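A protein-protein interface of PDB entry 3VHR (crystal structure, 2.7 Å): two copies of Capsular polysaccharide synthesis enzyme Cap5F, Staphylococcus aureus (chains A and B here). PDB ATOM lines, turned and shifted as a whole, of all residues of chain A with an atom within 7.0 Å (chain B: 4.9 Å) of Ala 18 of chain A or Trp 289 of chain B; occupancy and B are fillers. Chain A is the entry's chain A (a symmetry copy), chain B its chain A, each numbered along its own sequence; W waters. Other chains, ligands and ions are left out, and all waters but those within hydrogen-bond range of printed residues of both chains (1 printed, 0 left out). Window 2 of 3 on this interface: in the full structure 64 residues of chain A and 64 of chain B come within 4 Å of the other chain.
Water W1 bridges the side-chain hydroxyl of Ser 22 of chain A (2.7 Å) and the indole nitrogen of Trp 289 of chain B (2.9 Å).
Hydrophobic or aromatic side chains of chain A that line the printed part of chain B: Ala 18 and Trp 137. Printed residues of chain B that touch a printed residue of chain A: Trp 289, His 291, Gly 334 and Tyr 365. Hydrophobic or aromatic side chains of chain B within 4 Å of the printed part of chain A: Trp 289, His 291 and Tyr 365. Among the printed residues, 6 pairs touch across the chains. Among the printed residues, no Asp or Glu carboxylate lies within 4 Å of a Lys or Arg side-chain nitrogen of the other chain.
Among the printed residues, merely in contact across the chains: Ala 18 of chain A with Trp 289 of chain B (3.9 Å), Ser 22 of chain A with Trp 289 of chain B (3.5 Å), Thr 23 of chain A with Tyr 365 of chain B (3.4 Å) and Trp 137 of chain A with Gly 334 of chain B (3.9 Å).
No position is printed for both chains. Of the 6 pairs that touch across the chains among the printed residues, none has its exchanged pair printed and touching as well.
A ring nitrogen (ND1) of His 291 of chain B is in hydrogen-bond range of the side-chain amino group of Lys 136 of chain A (2.9 Å). A ring nitrogen (NE2) of His 291 of chain B is in hydrogen-bond range of the side-chain carboxylate (OD2) of Asp 19 of chain A.
Gly 13 of chain A touches none of the printed residues of chain B. Of the printed residues of chain B, Thr 23 of chain A touches Tyr 365 (3.4 Å). Of the printed residues of chain B, Lys 136 of chain A touches His 291. Asn 287 of chain B touches none of the printed residues of chain A. Trp 289 of chain B touches just these residues of chain A: Ala 18 (3.9 Å) and Ser 22 (3.5 Å). Of the printed residues of chain A, Gly 334 of chain B touches Trp 137. The nearest residue of chain A that does not touch Trp 289 of chain B is Lys 136 of chain A (4.4 Å).
The backbone carbonyl oxygen (O) of Ala 18 of chain A lies within hydrogen-bond range of the side-chain hydroxyl (OG) of Ser 22 of chain A. The side-chain amide oxygen (OD1) of Asn 15 of chain A is in hydrogen-bond range of the side-chain amino group (NZ) of Lys 136 of chain A (2.9 Å). The backbone NH of Trp 289 of chain B sits at hydrogen-bond distance from the backbone carbonyl oxygen of Tyr 365 of chain B (3.0 Å). The side-chain hydroxyl (OH) of Tyr 365 of chain B is in hydrogen-bond range of the side-chain carboxylate (OD1) of Asp 363 of chain B, 2.9 Å away. OD1 of Asp 363 of chain B sits at hydrogen-bond distance from N of His 291 of chain B, 3.0 Å away. OG1 of Thr 23 of chain A lies within hydrogen-bond range of O of Asp 19 of chain A (2.7 Å).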
ATOM      1  N   ILE A   5      30.923   5.501  14.067  1.00  0.00           N
ATOM      2  CA  ILE A   5      29.684   4.935  14.567  1.00  0.00           C
ATOM      3  C   ILE A   5      30.041   3.985  15.686  1.00  0.00           C
ATOM      4  O   ILE A   5      30.699   2.964  15.459  1.00  0.00           O
ATOM      5  CB  ILE A   5      28.937   4.171  13.454  1.00  0.00           C
ATOM      6  CG1 ILE A   5      28.650   5.088  12.267  1.00  0.00           C
ATOM      7  CG2 ILE A   5      27.645   3.584  13.984  1.00  0.00           C
ATOM      8  CD1 ILE A   5      28.557   4.357  10.953  1.00  0.00           C
ATOM      9  N   VAL A  12      20.568  -0.500  14.757  1.00  0.00           N
ATOM     10  CA  VAL A  12      20.650   0.770  14.035  1.00  0.00           C
ATOM     11  C   VAL A  12      21.997   0.854  13.312  1.00  0.00           C
ATOM     12  O   VAL A  12      22.063   1.227  12.136  1.00  0.00           O
ATOM     13  CB  VAL A  12      20.449   1.983  14.981  1.00  0.00           C
ATOM     14  CG1 VAL A  12      20.537   3.296  14.227  1.00  0.00           C
ATOM     15  CG2 VAL A  12      19.108   1.901  15.671  1.00  0.00           C
ATOM     16  N   GLY A  13      23.059   0.460  14.012  1.00  0.00           N
ATOM     17  CA  GLY A  13      24.420   0.513  13.476  1.00  0.00           C
ATOM     18  C   GLY A  13      24.614  -0.079  12.093  1.00  0.00           C
ATOM     19  O   GLY A  13      25.072   0.601  11.167  1.00  0.00           O
ATOM     20  N   LYS A  14      24.264  -1.356  11.966  1.00  0.00           N
ATOM     21  CA  LYS A  14      24.302  -2.052  10.689  1.00  0.00           C
ATOM     22  C   LYS A  14      23.414  -1.359   9.646  1.00  0.00           C
ATOM     23  O   LYS A  14      23.781  -1.284   8.483  1.00  0.00           O
ATOM     24  CB  LYS A  14      23.901  -3.516  10.872  1.00  0.00           C
ATOM     25  CG  LYS A  14      24.920  -4.342  11.654  1.00  0.00           C
ATOM     26  CD  LYS A  14      24.519  -5.809  11.804  1.00  0.00           C
ATOM     27  CE  LYS A  14      23.275  -5.974  12.679  1.00  0.00           C
ATOM     28  NZ  LYS A  14      23.309  -7.187  13.557  1.00  0.00           N
ATOM     29  N   ASN A  15      22.263  -0.839  10.057  1.00  0.00           N
ATOM     30  CA  ASN A  15      21.368  -0.166   9.112  1.00  0.00           C
ATOM     31  C   ASN A  15      21.951   1.140   8.592  1.00  0.00           C
ATOM     32  O   ASN A  15      22.047   1.356   7.382  1.00  0.00           O
ATOM     33  CB  ASN A  15      19.980   0.056   9.733  1.00  0.00           C
ATOM     34  CG  ASN A  15      19.102  -1.173   9.639  1.00  0.00           C
ATOM     35  OD1 ASN A  15      18.593  -1.493   8.572  1.00  0.00           O
ATOM     36  ND2 ASN A  15      18.930  -1.873  10.748  1.00  0.00           N
ATOM     37  N   LEU A  16      22.362   1.998   9.518  1.00  0.00           N
ATOM     38  CA  LEU A  16      23.058   3.231   9.180  1.00  0.00           C
ATOM     39  C   LEU A  16      24.294   3.007   8.301  1.00  0.00           C
ATOM     40  O   LEU A  16      24.488   3.696   7.316  1.00  0.00           O
ATOM     41  CB  LEU A  16      23.448   3.979  10.455  1.00  0.00           C
ATOM     42  CG  LEU A  16      23.997   5.391  10.239  1.00  0.00           C
ATOM     43  CD1 LEU A  16      22.971   6.292   9.558  1.00  0.00           C
ATOM     44  CD2 LEU A  16      24.475   5.985  11.547  1.00  0.00           C
ATOM     45  N   LYS A  17      25.125   2.046   8.666  1.00  0.00           N
ATOM     46  CA  LYS A  17      26.361   1.790   7.945  1.00  0.00           C
ATOM     47  C   LYS A  17      26.077   1.398   6.500  1.00  0.00           C
ATOM     48  O   LYS A  17      26.639   1.980   5.567  1.00  0.00           O
ATOM     49  CB  LYS A  17      27.170   0.705   8.665  1.00  0.00           C
ATOM     50  CG  LYS A  17      28.579   0.505   8.147  1.00  0.00           C
ATOM     51  CD  LYS A  17      28.594  -0.463   6.976  1.00  0.00           C
ATOM     52  CE  LYS A  17      30.005  -0.719   6.475  1.00  0.00           C
ATOM     53  NZ  LYS A  17      30.017  -2.009   5.731  1.00  0.00           N
ATOM     54  N   ALA A  18      25.209   0.404   6.333  1.00  0.00           N
ATOM     55  CA  ALA A  18      24.821  -0.085   5.031  1.00  0.00           C
ATOM     56  C   ALA A  18      24.312   1.073   4.200  1.00  0.00           C
ATOM     57  O   ALA A  18      24.730   1.262   3.061  1.00  0.00           O
ATOM     58  CB  ALA A  18      23.756  -1.146   5.171  1.00  0.00           C
ATOM     59  N   ASP A  19      23.437   1.875   4.784  1.00  0.00           N
ATOM     60  CA  ASP A  19      22.924   3.036   4.088  1.00  0.00           C
ATOM     61  C   ASP A  19      23.999   4.085   3.751  1.00  0.00           C
ATOM     62  O   ASP A  19      24.043   4.601   2.625  1.00  0.00           O
ATOM     63  CB  ASP A  19      21.785   3.674   4.882  1.00  0.00           C
ATOM     64  CG  ASP A  19      21.128   4.810   4.131  1.00  0.00           C
ATOM     65  OD1 ASP A  19      21.738   5.892   4.038  1.00  0.00           O
ATOM     66  OD2 ASP A  19      20.009   4.622   3.620  1.00  0.00           O
ATOM     67  N   LEU A  20      24.844   4.409   4.723  1.00  0.00           N
ATOM     68  CA  LEU A  20      25.872   5.422   4.539  1.00  0.00           C
ATOM     69  C   LEU A  20      26.942   5.068   3.497  1.00  0.00           C
ATOM     70  O   LEU A  20      27.397   5.956   2.769  1.00  0.00           O
ATOM     71  CB  LEU A  20      26.511   5.776   5.878  1.00  0.00           C
ATOM     72  CG  LEU A  20      26.256   7.154   6.493  1.00  0.00           C
ATOM     73  CD1 LEU A  20      24.957   7.806   6.048  1.00  0.00           C
ATOM     74  CD2 LEU A  20      26.318   7.013   8.003  1.00  0.00           C
ATOM     75  N   THR A  21      27.338   3.796   3.417  1.00  0.00           N
ATOM     76  CA  THR A  21      28.310   3.394   2.397  1.00  0.00           C
ATOM     77  C   THR A  21      27.692   3.341   0.995  1.00  0.00           C
ATOM     78  O   THR A  21      28.412   3.439  -0.003  1.00  0.00           O
ATOM     79  CB  THR A  21      29.079   2.086   2.729  1.00  0.00           C
ATOM     80  OG1 THR A  21      28.161   1.036   3.013  1.00  0.00           O
ATOM     81  CG2 THR A  21      29.985   2.276   3.943  1.00  0.00           C
ATOM     82  N   SER A  22      26.369   3.227   0.924  1.00  0.00           N
ATOM     83  CA  SER A  22      25.654   3.078  -0.349  1.00  0.00           C
ATOM     84  C   SER A  22      25.254   4.394  -0.989  1.00  0.00           C
ATOM     85  O   SER A  22      25.105   4.462  -2.204  1.00  0.00           O
ATOM     86  CB  SER A  22      24.376   2.254  -0.157  1.00  0.00           C
ATOM     87  OG  SER A  22      24.673   0.960   0.324  1.00  0.00           O
ATOM     88  N   THR A  23      25.044   5.424  -0.171  1.00  0.00           N
ATOM     89  CA  THR A  23      24.412   6.658  -0.643  1.00  0.00           C
ATOM     90  C   THR A  23      25.179   7.936  -0.358  1.00  0.00           C
ATOM     91  O   THR A  23      24.680   9.015  -0.647  1.00  0.00           O
ATOM     92  CB  THR A  23      22.987   6.837  -0.069  1.00  0.00           C
ATOM     93  OG1 THR A  23      23.013   6.773   1.369  1.00  0.00           O
ATOM     94  CG2 THR A  23      22.075   5.789  -0.608  1.00  0.00           C
ATOM     95  N   GLU A  30      33.779   2.308  11.689  1.00  0.00           N
ATOM     96  CA  GLU A  30      32.934   1.525  12.595  1.00  0.00           C
ATOM     97  C   GLU A  30      33.706   1.135  13.842  1.00  0.00           C
ATOM     98  O   GLU A  30      34.796   0.570  13.737  1.00  0.00           O
ATOM     99  CB  GLU A  30      32.475   0.225  11.932  1.00  0.00           C
ATOM    100  CG  GLU A  30      31.486   0.320  10.786  1.00  0.00           C
ATOM    101  CD  GLU A  30      31.546  -0.931   9.923  1.00  0.00           C
ATOM    102  OE1 GLU A  30      30.561  -1.689   9.892  1.00  0.00           O
ATOM    103  OE2 GLU A  30      32.599  -1.185   9.295  1.00  0.00           O
ATOM    104  N   LYS A 136      14.346  -4.304   9.836  1.00  0.00           N
ATOM    105  CA  LYS A 136      15.207  -5.454   9.540  1.00  0.00           C
ATOM    106  C   LYS A 136      16.475  -5.507  10.405  1.00  0.00           C
ATOM    107  O   LYS A 136      16.982  -4.477  10.848  1.00  0.00           O
ATOM    108  CB  LYS A 136      15.580  -5.486   8.060  1.00  0.00           C
ATOM    109  CG  LYS A 136      16.315  -4.254   7.567  1.00  0.00           C
ATOM    110  CD  LYS A 136      16.305  -4.184   6.050  1.00  0.00           C
ATOM    111  CE  LYS A 136      17.390  -3.239   5.560  1.00  0.00           C
ATOM    112  NZ  LYS A 136      17.105  -1.878   6.071  1.00  0.00           N
ATOM    113  N   TRP A 137      16.964  -6.722  10.649  1.00  0.00           N
ATOM    114  CA  TRP A 137      18.253  -6.945  11.325  1.00  0.00           C
ATOM    115  C   TRP A 137      18.263  -6.769  12.828  1.00  0.00           C
ATOM    116  O   TRP A 137      19.319  -6.860  13.450  1.00  0.00           O
ATOM    117  CB  TRP A 137      19.377  -6.116  10.675  1.00  0.00           C
ATOM    118  CG  TRP A 137      19.443  -6.243   9.170  1.00  0.00           C
ATOM    119  CD1 TRP A 137      18.875  -7.237   8.368  1.00  0.00           C
ATOM    120  CD2 TRP A 137      20.157  -5.366   8.235  1.00  0.00           C
ATOM    121  NE1 TRP A 137      19.161  -7.022   7.041  1.00  0.00           N
ATOM    122  CE2 TRP A 137      19.933  -5.923   6.894  1.00  0.00           C
ATOM    123  CE3 TRP A 137      20.922  -4.214   8.368  1.00  0.00           C
ATOM    124  CZ2 TRP A 137      20.457  -5.332   5.759  1.00  0.00           C
ATOM    125  CZ3 TRP A 137      21.446  -3.624   7.212  1.00  0.00           C
ATOM    126  CH2 TRP A 137      21.217  -4.171   5.940  1.00  0.00           C
ATOM    127  N   ASN B 287      20.757  -7.200  -9.253  1.00  0.00           N
ATOM    128  CA  ASN B 287      21.945  -6.948  -8.437  1.00  0.00           C
ATOM    129  C   ASN B 287      21.794  -5.692  -7.579  1.00  0.00           C
ATOM    130  O   ASN B 287      22.723  -4.896  -7.467  1.00  0.00           O
ATOM    131  CB  ASN B 287      23.207  -6.852  -9.297  1.00  0.00           C
ATOM    132  CG  ASN B 287      23.656  -8.196  -9.831  1.00  0.00           C
ATOM    133  OD1 ASN B 287      23.748  -9.186  -9.101  1.00  0.00           O
ATOM    134  ND2 ASN B 287      23.957  -8.234 -11.118  1.00  0.00           N
ATOM    135  N   HIS B 288      20.619  -5.512  -6.982  1.00  0.00           N
ATOM    136  CA  HIS B 288      20.412  -4.419  -6.041  1.00  0.00           C
ATOM    137  C   HIS B 288      19.713  -4.852  -4.772  1.00  0.00           C
ATOM    138  O   HIS B 288      19.194  -5.966  -4.672  1.00  0.00           O
ATOM    139  CB  HIS B 288      19.704  -3.238  -6.716  1.00  0.00           C
ATOM    140  CG  HIS B 288      18.428  -3.604  -7.470  1.00  0.00           C
ATOM    141  ND1 HIS B 288      18.202  -3.215  -8.742  1.00  0.00           N
ATOM    142  CD2 HIS B 288      17.285  -4.312  -7.069  1.00  0.00           C
ATOM    143  CE1 HIS B 288      16.992  -3.660  -9.141  1.00  0.00           C
ATOM    144  NE2 HIS B 288      16.429  -4.327  -8.117  1.00  0.00           N
ATOM    145  N   TRP B 289      19.715  -3.999  -3.761  1.00  0.00           N
ATOM    146  CA  TRP B 289      18.897  -4.282  -2.587  1.00  0.00           C
ATOM    147  C   TRP B 289      18.084  -3.075  -2.211  1.00  0.00           C
ATOM    148  O   TRP B 289      18.348  -1.963  -2.687  1.00  0.00           O
ATOM    149  CB  TRP B 289      19.738  -4.816  -1.425  1.00  0.00           C
ATOM    150  CG  TRP B 289      20.774  -3.853  -0.917  1.00  0.00           C
ATOM    151  CD1 TRP B 289      22.034  -3.596  -1.447  1.00  0.00           C
ATOM    152  CD2 TRP B 289      20.671  -2.989   0.261  1.00  0.00           C
ATOM    153  NE1 TRP B 289      22.693  -2.656  -0.698  1.00  0.00           N
ATOM    154  CE2 TRP B 289      21.931  -2.249   0.336  1.00  0.00           C
ATOM    155  CE3 TRP B 289      19.691  -2.757   1.223  1.00  0.00           C
ATOM    156  CZ2 TRP B 289      22.175  -1.321   1.335  1.00  0.00           C
ATOM    157  CZ3 TRP B 289      19.949  -1.831   2.225  1.00  0.00           C
ATOM    158  CH2 TRP B 289      21.161  -1.129   2.281  1.00  0.00           C
ATOM    159  N   HIS B 290      17.072  -3.290  -1.377  1.00  0.00           N
ATOM    160  CA  HIS B 290      16.176  -2.223  -0.963  1.00  0.00           C
ATOM    161  C   HIS B 290      16.103  -2.162   0.527  1.00  0.00           C
ATOM    162  O   HIS B 290      16.282  -3.180   1.188  1.00  0.00           O
ATOM    163  CB  HIS B 290      14.771  -2.485  -1.501  1.00  0.00           C
ATOM    164  CG  HIS B 290      14.715  -2.782  -2.979  1.00  0.00           C
ATOM    165  ND1 HIS B 290      15.026  -1.870  -3.918  1.00  0.00           N
ATOM    166  CD2 HIS B 290      14.328  -3.930  -3.660  1.00  0.00           C
ATOM    167  CE1 HIS B 290      14.866  -2.411  -5.139  1.00  0.00           C
ATOM    168  NE2 HIS B 290      14.434  -3.672  -4.982  1.00  0.00           N
ATOM    169  N   HIS B 291      15.812  -0.979   1.069  1.00  0.00           N
ATOM    170  CA  HIS B 291      15.527  -0.850   2.499  1.00  0.00           C
ATOM    171  C   HIS B 291      14.146  -1.323   2.819  1.00  0.00           C
ATOM    172  O   HIS B 291      13.970  -2.149   3.708  1.00  0.00           O
ATOM    173  CB  HIS B 291      15.648   0.591   2.979  1.00  0.00           C
ATOM    174  CG  HIS B 291      17.038   0.987   3.413  1.00  0.00           C
ATOM    175  ND1 HIS B 291      17.785   0.231   4.237  1.00  0.00           N
ATOM    176  CD2 HIS B 291      17.792   2.125   3.133  1.00  0.00           C
ATOM    177  CE1 HIS B 291      18.965   0.837   4.462  1.00  0.00           C
ATOM    178  NE2 HIS B 291      18.970   1.996   3.784  1.00  0.00           N
ATOM    179  N   VAL B 311      22.800  -8.706   2.511  1.00  0.00           N
ATOM    180  CA  VAL B 311      23.796  -7.634   2.413  1.00  0.00           C
ATOM    181  C   VAL B 311      25.058  -7.860   3.274  1.00  0.00           C
ATOM    182  O   VAL B 311      26.169  -7.532   2.854  1.00  0.00           O
ATOM    183  CB  VAL B 311      23.154  -6.254   2.729  1.00  0.00           C
ATOM    184  CG1 VAL B 311      24.210  -5.191   3.001  1.00  0.00           C
ATOM    185  CG2 VAL B 311      22.263  -5.805   1.587  1.00  0.00           C
ATOM    186  N   GLY B 334      16.593  -6.003   2.396  1.00  0.00           N
ATOM    187  CA  GLY B 334      17.937  -6.265   2.880  1.00  0.00           C
ATOM    188  C   GLY B 334      18.697  -7.397   2.208  1.00  0.00           C
ATOM    189  O   GLY B 334      19.816  -7.706   2.622  1.00  0.00           O
ATOM    190  N   TYR B 335      18.097  -8.024   1.194  1.00  0.00           N
ATOM    191  CA  TYR B 335      18.797  -9.020   0.371  1.00  0.00           C
ATOM    192  C   TYR B 335      19.016  -8.458  -0.998  1.00  0.00           C
ATOM    193  O   TYR B 335      18.063  -8.055  -1.679  1.00  0.00           O
ATOM    194  CB  TYR B 335      18.001 -10.310   0.215  1.00  0.00           C
ATOM    195  CG  TYR B 335      17.929 -11.149   1.452  1.00  0.00           C
ATOM    196  CD1 TYR B 335      17.029 -10.838   2.470  1.00  0.00           C
ATOM    197  CD2 TYR B 335      18.757 -12.252   1.615  1.00  0.00           C
ATOM    198  CE1 TYR B 335      16.952 -11.596   3.619  1.00  0.00           C
ATOM    199  CE2 TYR B 335      18.697 -13.022   2.767  1.00  0.00           C
ATOM    200  CZ  TYR B 335      17.785 -12.687   3.763  1.00  0.00           C
ATOM    201  OH  TYR B 335      17.695 -13.437   4.906  1.00  0.00           O
ATOM    202  N   THR B 336      20.273  -8.427  -1.417  1.00  0.00           N
ATOM    203  CA  THR B 336      20.547  -8.100  -2.805  1.00  0.00           C
ATOM    204  C   THR B 336      20.032  -9.245  -3.679  1.00  0.00           C
ATOM    205  O   THR B 336      20.090 -10.414  -3.269  1.00  0.00           O
ATOM    206  CB  THR B 336      22.022  -7.771  -3.066  1.00  0.00           C
ATOM    207  OG1 THR B 336      22.119  -7.180  -4.362  1.00  0.00           O
ATOM    208  CG2 THR B 336      22.906  -9.015  -2.992  1.00  0.00           C
ATOM    209  N   HIS B 337      19.499  -8.908  -4.851  1.00  0.00           N
ATOM    210  CA  HIS B 337      18.833  -9.903  -5.685  1.00  0.00           C
ATOM    211  C   HIS B 337      19.000  -9.695  -7.155  1.00  0.00           C
ATOM    212  O   HIS B 337      18.980  -8.565  -7.625  1.00  0.00           O
ATOM    213  CB  HIS B 337      17.361  -9.972  -5.344  1.00  0.00           C
ATOM    214  CG  HIS B 337      16.691  -8.623  -5.268  1.00  0.00           C
ATOM    215  ND1 HIS B 337      16.782  -7.830  -4.184  1.00  0.00           N
ATOM    216  CD2 HIS B 337      15.896  -7.943  -6.188  1.00  0.00           C
ATOM    217  CE1 HIS B 337      16.086  -6.702  -4.403  1.00  0.00           C
ATOM    218  NE2 HIS B 337      15.548  -6.773  -5.627  1.00  0.00           N
ATOM    219  N   ASP B 363      15.252   4.075  -3.381  1.00  0.00           N
ATOM    220  CA  ASP B 363      15.478   3.002  -2.414  1.00  0.00           C
ATOM    221  C   ASP B 363      15.991   1.718  -3.093  1.00  0.00           C
ATOM    222  O   ASP B 363      15.472   0.608  -2.900  1.00  0.00           O
ATOM    223  CB  ASP B 363      14.215   2.739  -1.593  1.00  0.00           C
ATOM    224  CG  ASP B 363      14.465   1.804  -0.442  1.00  0.00           C
ATOM    225  OD1 ASP B 363      15.598   1.845   0.095  1.00  0.00           O
ATOM    226  OD2 ASP B 363      13.546   1.023  -0.099  1.00  0.00           O
ATOM    227  N   THR B 364      17.017   1.886  -3.908  1.00  0.00           N
ATOM    228  CA  THR B 364      17.615   0.764  -4.606  1.00  0.00           C
ATOM    229  C   THR B 364      19.113   1.028  -4.764  1.00  0.00           C
ATOM    230  O   THR B 364      19.528   2.063  -5.286  1.00  0.00           O
ATOM    231  CB  THR B 364      16.834   0.390  -5.912  1.00  0.00           C
ATOM    232  OG1 THR B 364      17.686  -0.307  -6.822  1.00  0.00           O
ATOM    233  CG2 THR B 364      16.291   1.584  -6.601  1.00  0.00           C
ATOM    234  N   TYR B 365      19.914   0.097  -4.248  1.00  0.00           N
ATOM    235  CA  TYR B 365      21.368   0.273  -4.095  1.00  0.00           C
ATOM    236  C   TYR B 365      22.112  -0.882  -4.743  1.00  0.00           C
ATOM    237  O   TYR B 365      21.903  -2.046  -4.387  1.00  0.00           O
ATOM    238  CB  TYR B 365      21.733   0.390  -2.612  1.00  0.00           C
ATOM    239  CG  TYR B 365      20.741   1.223  -1.832  1.00  0.00           C
ATOM    240  CD1 TYR B 365      20.711   2.610  -1.963  1.00  0.00           C
ATOM    241  CD2 TYR B 365      19.809   0.624  -0.997  1.00  0.00           C
ATOM    242  CE1 TYR B 365      19.793   3.380  -1.277  1.00  0.00           C
ATOM    243  CE2 TYR B 365      18.876   1.385  -0.303  1.00  0.00           C
ATOM    244  CZ  TYR B 365      18.878   2.767  -0.447  1.00  0.00           C
ATOM    245  OH  TYR B 365      17.961   3.533   0.243  1.00  0.00           O
ATOM    246  N   LEU B 367      24.484  -3.734  -5.699  1.00  0.00           N
ATOM    247  CA  LEU B 367      25.356  -4.698  -5.010  1.00  0.00           C
ATOM    248  C   LEU B 367      25.367  -6.028  -5.756  1.00  0.00           C
ATOM    249  O   LEU B 367      24.323  -6.643  -5.964  1.00  0.00           O
ATOM    250  CB  LEU B 367      24.918  -4.927  -3.559  1.00  0.00           C
ATOM    251  CG  LEU B 367      25.850  -5.765  -2.668  1.00  0.00           C
ATOM    252  CD1 LEU B 367      27.049  -4.958  -2.181  1.00  0.00           C
ATOM    253  CD2 LEU B 367      25.076  -6.331  -1.490  1.00  0.00           C
HETATM  254  O   HOH W   1      25.238  -1.356  -1.023  1.00  0.00           O
